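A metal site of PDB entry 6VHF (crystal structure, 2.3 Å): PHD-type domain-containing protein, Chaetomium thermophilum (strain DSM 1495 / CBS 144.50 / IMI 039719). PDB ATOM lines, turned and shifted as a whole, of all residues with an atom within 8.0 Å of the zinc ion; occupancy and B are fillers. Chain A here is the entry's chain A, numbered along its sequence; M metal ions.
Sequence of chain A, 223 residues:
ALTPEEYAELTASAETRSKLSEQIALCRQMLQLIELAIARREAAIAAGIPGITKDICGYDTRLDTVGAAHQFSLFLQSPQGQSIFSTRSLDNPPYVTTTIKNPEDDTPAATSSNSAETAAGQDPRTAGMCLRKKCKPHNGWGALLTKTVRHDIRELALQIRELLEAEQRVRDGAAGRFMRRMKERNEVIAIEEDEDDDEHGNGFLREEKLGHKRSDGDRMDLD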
ATOM      1  N   ASP A  55      11.992  33.190  29.582  1.00  0.00           N
ATOM      2  CA  ASP A  55      10.770  32.421  29.725  1.00  0.00           C
ATOM      3  C   ASP A  55      10.520  31.498  28.546  1.00  0.00           C
ATOM      4  O   ASP A  55       9.563  30.713  28.582  1.00  0.00           O
ATOM      5  CB  ASP A  55       9.562  33.364  29.891  1.00  0.00           C
ATOM      6  CG  ASP A  55       9.749  34.381  30.989  1.00  0.00           C
ATOM      7  OD1 ASP A  55       9.574  35.592  30.718  1.00  0.00           O
ATOM      8  OD2 ASP A  55      10.056  33.965  32.125  1.00  0.00           O
ATOM      9  N   ILE A  56      11.319  31.619  27.473  1.00  0.00           N
ATOM     10  CA  ILE A  56      11.103  30.795  26.281  1.00  0.00           C
ATOM     11  C   ILE A  56      11.213  29.319  26.624  1.00  0.00           C
ATOM     12  O   ILE A  56      12.112  28.895  27.358  1.00  0.00           O
ATOM     13  CB  ILE A  56      12.130  31.205  25.200  1.00  0.00           C
ATOM     14  CG1 ILE A  56      11.587  32.361  24.368  1.00  0.00           C
ATOM     15  CG2 ILE A  56      12.512  30.003  24.322  1.00  0.00           C
ATOM     16  CD1 ILE A  56      10.340  32.025  23.608  1.00  0.00           C
ATOM     17  N   CYS A  57      10.266  28.524  26.101  1.00  0.00           N
ATOM     18  CA  CYS A  57      10.262  27.077  26.334  1.00  0.00           C
ATOM     19  C   CYS A  57      11.506  26.421  25.736  1.00  0.00           C
ATOM     20  O   CYS A  57      12.343  25.881  26.464  1.00  0.00           O
ATOM     21  CB  CYS A  57       8.996  26.452  25.740  1.00  0.00           C
ATOM     22  SG  CYS A  57       9.005  24.604  25.856  1.00  0.00           S
ATOM     23  N   GLY A  58      11.639  26.475  24.405  1.00  0.00           N
ATOM     24  CA  GLY A  58      12.844  26.010  23.751  1.00  0.00           C
ATOM     25  C   GLY A  58      12.831  24.553  23.336  1.00  0.00           C
ATOM     26  O   GLY A  58      13.800  24.100  22.714  1.00  0.00           O
ATOM     27  N   TYR A  59      11.766  23.826  23.650  1.00  0.00           N
ATOM     28  CA  TYR A  59      11.621  22.428  23.246  1.00  0.00           C
ATOM     29  C   TYR A  59      11.800  22.276  21.743  1.00  0.00           C
ATOM     30  O   TYR A  59      11.158  22.960  20.956  1.00  0.00           O
ATOM     31  CB  TYR A  59      10.241  21.920  23.692  1.00  0.00           C
ATOM     32  CG  TYR A  59       9.988  20.458  23.483  1.00  0.00           C
ATOM     33  CD1 TYR A  59       9.387  20.001  22.313  1.00  0.00           C
ATOM     34  CD2 TYR A  59      10.310  19.524  24.452  1.00  0.00           C
ATOM     35  CE1 TYR A  59       9.124  18.680  22.113  1.00  0.00           C
ATOM     36  CE2 TYR A  59      10.052  18.182  24.262  1.00  0.00           C
ATOM     37  CZ  TYR A  59       9.456  17.765  23.087  1.00  0.00           C
ATOM     38  OH  TYR A  59       9.194  16.415  22.875  1.00  0.00           O
ATOM     39  N   ASP A  60      12.694  21.369  21.361  1.00  0.00           N
ATOM     40  CA  ASP A  60      12.942  21.039  19.964  1.00  0.00           C
ATOM     41  C   ASP A  60      12.014  19.911  19.519  1.00  0.00           C
ATOM     42  O   ASP A  60      11.793  18.930  20.245  1.00  0.00           O
ATOM     43  CB  ASP A  60      14.407  20.614  19.799  1.00  0.00           C
ATOM     44  CG  ASP A  60      14.867  20.656  18.368  1.00  0.00           C
ATOM     45  OD1 ASP A  60      14.289  19.921  17.523  1.00  0.00           O
ATOM     46  OD2 ASP A  60      15.824  21.408  18.079  1.00  0.00           O
ATOM     47  N   MET A 129      11.893  25.113  17.179  1.00  0.00           N
ATOM     48  CA  MET A 129      11.926  25.411  18.597  1.00  0.00           C
ATOM     49  C   MET A 129      10.576  25.950  19.041  1.00  0.00           C
ATOM     50  O   MET A 129       9.937  26.718  18.314  1.00  0.00           O
ATOM     51  CB  MET A 129      13.047  26.421  18.895  1.00  0.00           C
ATOM     52  CG  MET A 129      13.478  26.497  20.338  1.00  0.00           C
ATOM     53  SD  MET A 129      14.649  27.845  20.649  1.00  0.00           S
ATOM     54  CE  MET A 129      16.137  27.287  19.825  1.00  0.00           C
ATOM     55  N   CYS A 130      10.136  25.530  20.215  1.00  0.00           N
ATOM     56  CA  CYS A 130       8.846  25.965  20.749  1.00  0.00           C
ATOM     57  C   CYS A 130       9.056  27.260  21.504  1.00  0.00           C
ATOM     58  O   CYS A 130       9.800  27.304  22.488  1.00  0.00           O
ATOM     59  CB  CYS A 130       8.243  24.917  21.678  1.00  0.00           C
ATOM     60  SG  CYS A 130       6.864  25.554  22.633  1.00  0.00           S
ATOM     61  N   LEU A 131       8.386  28.323  21.045  1.00  0.00           N
ATOM     62  CA  LEU A 131       8.588  29.660  21.604  1.00  0.00           C
ATOM     63  C   LEU A 131       7.521  30.057  22.621  1.00  0.00           C
ATOM     64  O   LEU A 131       7.420  31.236  22.970  1.00  0.00           O
ATOM     65  CB  LEU A 131       8.669  30.704  20.483  1.00  0.00           C
ATOM     66  CG  LEU A 131       9.889  30.730  19.556  1.00  0.00           C
ATOM     67  CD1 LEU A 131      11.197  30.427  20.317  1.00  0.00           C
ATOM     68  CD2 LEU A 131       9.701  29.783  18.370  1.00  0.00           C
ATOM     69  N   ARG A 132       6.730  29.101  23.113  1.00  0.00           N
ATOM     70  CA  ARG A 132       5.759  29.439  24.140  1.00  0.00           C
ATOM     71  C   ARG A 132       6.484  29.909  25.395  1.00  0.00           C
ATOM     72  O   ARG A 132       7.532  29.374  25.754  1.00  0.00           O
ATOM     73  CB  ARG A 132       4.844  28.252  24.421  1.00  0.00           C
ATOM     74  CG  ARG A 132       3.664  28.554  25.357  1.00  0.00           C
ATOM     75  CD  ARG A 132       2.464  29.229  24.638  1.00  0.00           C
ATOM     76  NE  ARG A 132       2.823  30.477  23.963  1.00  0.00           N
ATOM     77  CZ  ARG A 132       2.945  31.653  24.569  1.00  0.00           C
ATOM     78  NH1 ARG A 132       2.750  31.757  25.877  1.00  0.00           N
ATOM     79  NH2 ARG A 132       3.281  32.743  23.884  1.00  0.00           N
ATOM     80  N   LYS A 133       5.960  30.953  26.045  1.00  0.00           N
ATOM     81  CA  LYS A 133       6.514  31.403  27.315  1.00  0.00           C
ATOM     82  C   LYS A 133       5.757  30.726  28.454  1.00  0.00           C
ATOM     83  O   LYS A 133       4.552  30.515  28.381  1.00  0.00           O
ATOM     84  CB  LYS A 133       6.414  32.925  27.467  1.00  0.00           C
ATOM     85  CG  LYS A 133       7.404  33.738  26.600  1.00  0.00           C
ATOM     86  CD  LYS A 133       7.459  35.221  27.018  1.00  0.00           C
ATOM     87  CE  LYS A 133       8.246  36.081  26.029  1.00  0.00           C
ATOM     88  NZ  LYS A 133       7.849  35.859  24.603  1.00  0.00           N
ATOM     89  N   LYS A 134       6.496  30.389  29.516  1.00  0.00           N
ATOM     90  CA  LYS A 134       5.975  29.560  30.611  1.00  0.00           C
ATOM     91  C   LYS A 134       5.173  28.374  30.061  1.00  0.00           C
ATOM     92  O   LYS A 134       3.980  28.207  30.317  1.00  0.00           O
ATOM     93  CB  LYS A 134       5.132  30.391  31.571  1.00  0.00           C
ATOM     94  CG  LYS A 134       5.901  31.429  32.391  1.00  0.00           C
ATOM     95  CD  LYS A 134       6.127  32.709  31.600  1.00  0.00           C
ATOM     96  CE  LYS A 134       6.560  33.850  32.516  1.00  0.00           C
ATOM     97  NZ  LYS A 134       7.691  33.454  33.408  1.00  0.00           N
ATOM     98  N   CYS A 135       5.854  27.568  29.257  1.00  0.00           N
ATOM     99  CA  CYS A 135       5.166  26.492  28.549  1.00  0.00           C
ATOM    100  C   CYS A 135       4.829  25.344  29.498  1.00  0.00           C
ATOM    101  O   CYS A 135       5.545  25.087  30.479  1.00  0.00           O
ATOM    102  CB  CYS A 135       6.024  25.981  27.414  1.00  0.00           C
ATOM    103  SG  CYS A 135       5.268  24.645  26.550  1.00  0.00           S
ATOM    104  N   LYS A 136       3.729  24.665  29.204  1.00  0.00           N
ATOM    105  CA  LYS A 136       3.179  23.638  30.097  1.00  0.00           C
ATOM    106  C   LYS A 136       3.075  22.266  29.426  1.00  0.00           C
ATOM    107  O   LYS A 136       3.289  21.251  30.099  1.00  0.00           O
ATOM    108  CB  LYS A 136       1.814  24.076  30.642  1.00  0.00           C
ATOM    109  CG  LYS A 136       1.881  25.223  31.647  1.00  0.00           C
ATOM    110  CD  LYS A 136       3.128  25.133  32.525  1.00  0.00           C
ATOM    111  CE  LYS A 136       2.963  25.913  33.808  1.00  0.00           C
ATOM    112  NZ  LYS A 136       4.123  25.663  34.721  1.00  0.00           N
ATOM    113  N   PRO A 137       2.752  22.187  28.126  1.00  0.00           N
ATOM    114  CA  PRO A 137       2.912  20.901  27.430  1.00  0.00           C
ATOM    115  C   PRO A 137       4.344  20.355  27.465  1.00  0.00           C
ATOM    116  O   PRO A 137       4.534  19.125  27.436  1.00  0.00           O
ATOM    117  CB  PRO A 137       2.477  21.227  25.991  1.00  0.00           C
ATOM    118  CG  PRO A 137       1.505  22.336  26.152  1.00  0.00           C
ATOM    119  CD  PRO A 137       1.951  23.135  27.331  1.00  0.00           C
ATOM    120  N   HIS A 138       5.339  21.238  27.521  1.00  0.00           N
ATOM    121  CA  HIS A 138       6.746  20.851  27.594  1.00  0.00           C
ATOM    122  C   HIS A 138       7.381  21.280  28.905  1.00  0.00           C
ATOM    123  O   HIS A 138       8.606  21.366  29.013  1.00  0.00           O
ATOM    124  CB  HIS A 138       7.537  21.458  26.416  1.00  0.00           C
ATOM    125  CG  HIS A 138       6.919  21.233  25.076  1.00  0.00           C
ATOM    126  ND1 HIS A 138       6.927  22.187  24.083  1.00  0.00           N
ATOM    127  CD2 HIS A 138       6.287  20.154  24.549  1.00  0.00           C
ATOM    128  CE1 HIS A 138       6.319  21.719  23.015  1.00  0.00           C
ATOM    129  NE2 HIS A 138       5.927  20.489  23.267  1.00  0.00           N
ATOM    130  N   ASN A 139       6.564  21.570  29.917  1.00  0.00           N
ATOM    131  CA  ASN A 139       7.026  22.064  31.198  1.00  0.00           C
ATOM    132  C   ASN A 139       8.167  21.209  31.760  1.00  0.00           C
ATOM    133  O   ASN A 139       7.996  20.009  31.970  1.00  0.00           O
ATOM    134  CB  ASN A 139       5.851  22.090  32.173  1.00  0.00           C
ATOM    135  CG  ASN A 139       6.215  22.686  33.509  1.00  0.00           C
ATOM    136  OD1 ASN A 139       6.820  23.766  33.582  1.00  0.00           O
ATOM    137  ND2 ASN A 139       5.857  21.989  34.587  1.00  0.00           N
ATOM    138  N   GLY A 140       9.311  21.852  31.990  1.00  0.00           N
ATOM    139  CA  GLY A 140      10.463  21.165  32.571  1.00  0.00           C
ATOM    140  C   GLY A 140      11.056  20.057  31.716  1.00  0.00           C
ATOM    141  O   GLY A 140      11.522  19.049  32.260  1.00  0.00           O
ATOM    142  N   TRP A 141      11.073  20.220  30.395  1.00  0.00           N
ATOM    143  CA  TRP A 141      11.468  19.106  29.538  1.00  0.00           C
ATOM    144  C   TRP A 141      12.937  18.731  29.733  1.00  0.00           C
ATOM    145  O   TRP A 141      13.280  17.549  29.730  1.00  0.00           O
ATOM    146  CB  TRP A 141      11.174  19.425  28.074  1.00  0.00           C
ATOM    147  CG  TRP A 141      11.837  20.691  27.514  1.00  0.00           C
ATOM    148  CD1 TRP A 141      11.283  21.937  27.435  1.00  0.00           C
ATOM    149  CD2 TRP A 141      13.150  20.795  26.930  1.00  0.00           C
ATOM    150  NE1 TRP A 141      12.162  22.816  26.857  1.00  0.00           N
ATOM    151  CE2 TRP A 141      13.311  22.137  26.533  1.00  0.00           C
ATOM    152  CE3 TRP A 141      14.191  19.891  26.703  1.00  0.00           C
ATOM    153  CZ2 TRP A 141      14.490  22.596  25.924  1.00  0.00           C
ATOM    154  CZ3 TRP A 141      15.344  20.340  26.107  1.00  0.00           C
ATOM    155  CH2 TRP A 141      15.494  21.692  25.718  1.00  0.00           C
HETATM  156 ZN    ZN M   1       6.837  24.205  24.864  1.00  0.00          ZN
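N of Tyr 59 lies close to SG of Cys 57 (3.6 Å). N of Cys 57 sits at hydrogen-bond distance from O of Arg 132 (2.9 Å). O of Cys 57 lies within hydrogen-bond range of NE1 of Trp 141 (3.1 Å). The backbone NH (N) of Cys 130 sits at hydrogen-bond distance from the backbone carbonyl oxygen (O) of Tyr 59 (2.9 Å). The backbone NH of Arg 132 sits close to the side-chain sulfur of Cys 130. O of Cys 130 is in hydrogen-bond range of N of Gly 58 (2.8 Å).
The nearest printed residue that does not touch the zinc ion is Tyr 59 (4.3 Å).
ND1 of His 138 is bound to the zinc ion (2.2 Å). The zinc ion is bound by SG of Cys 135, 2.3 Å away. The zinc ion is bound by the side-chain sulfur (SG) of Cys 57 (2.4 Å). The side-chain sulfur (SG) of Cys 130 is bound to the zinc ion (2.6 Å).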
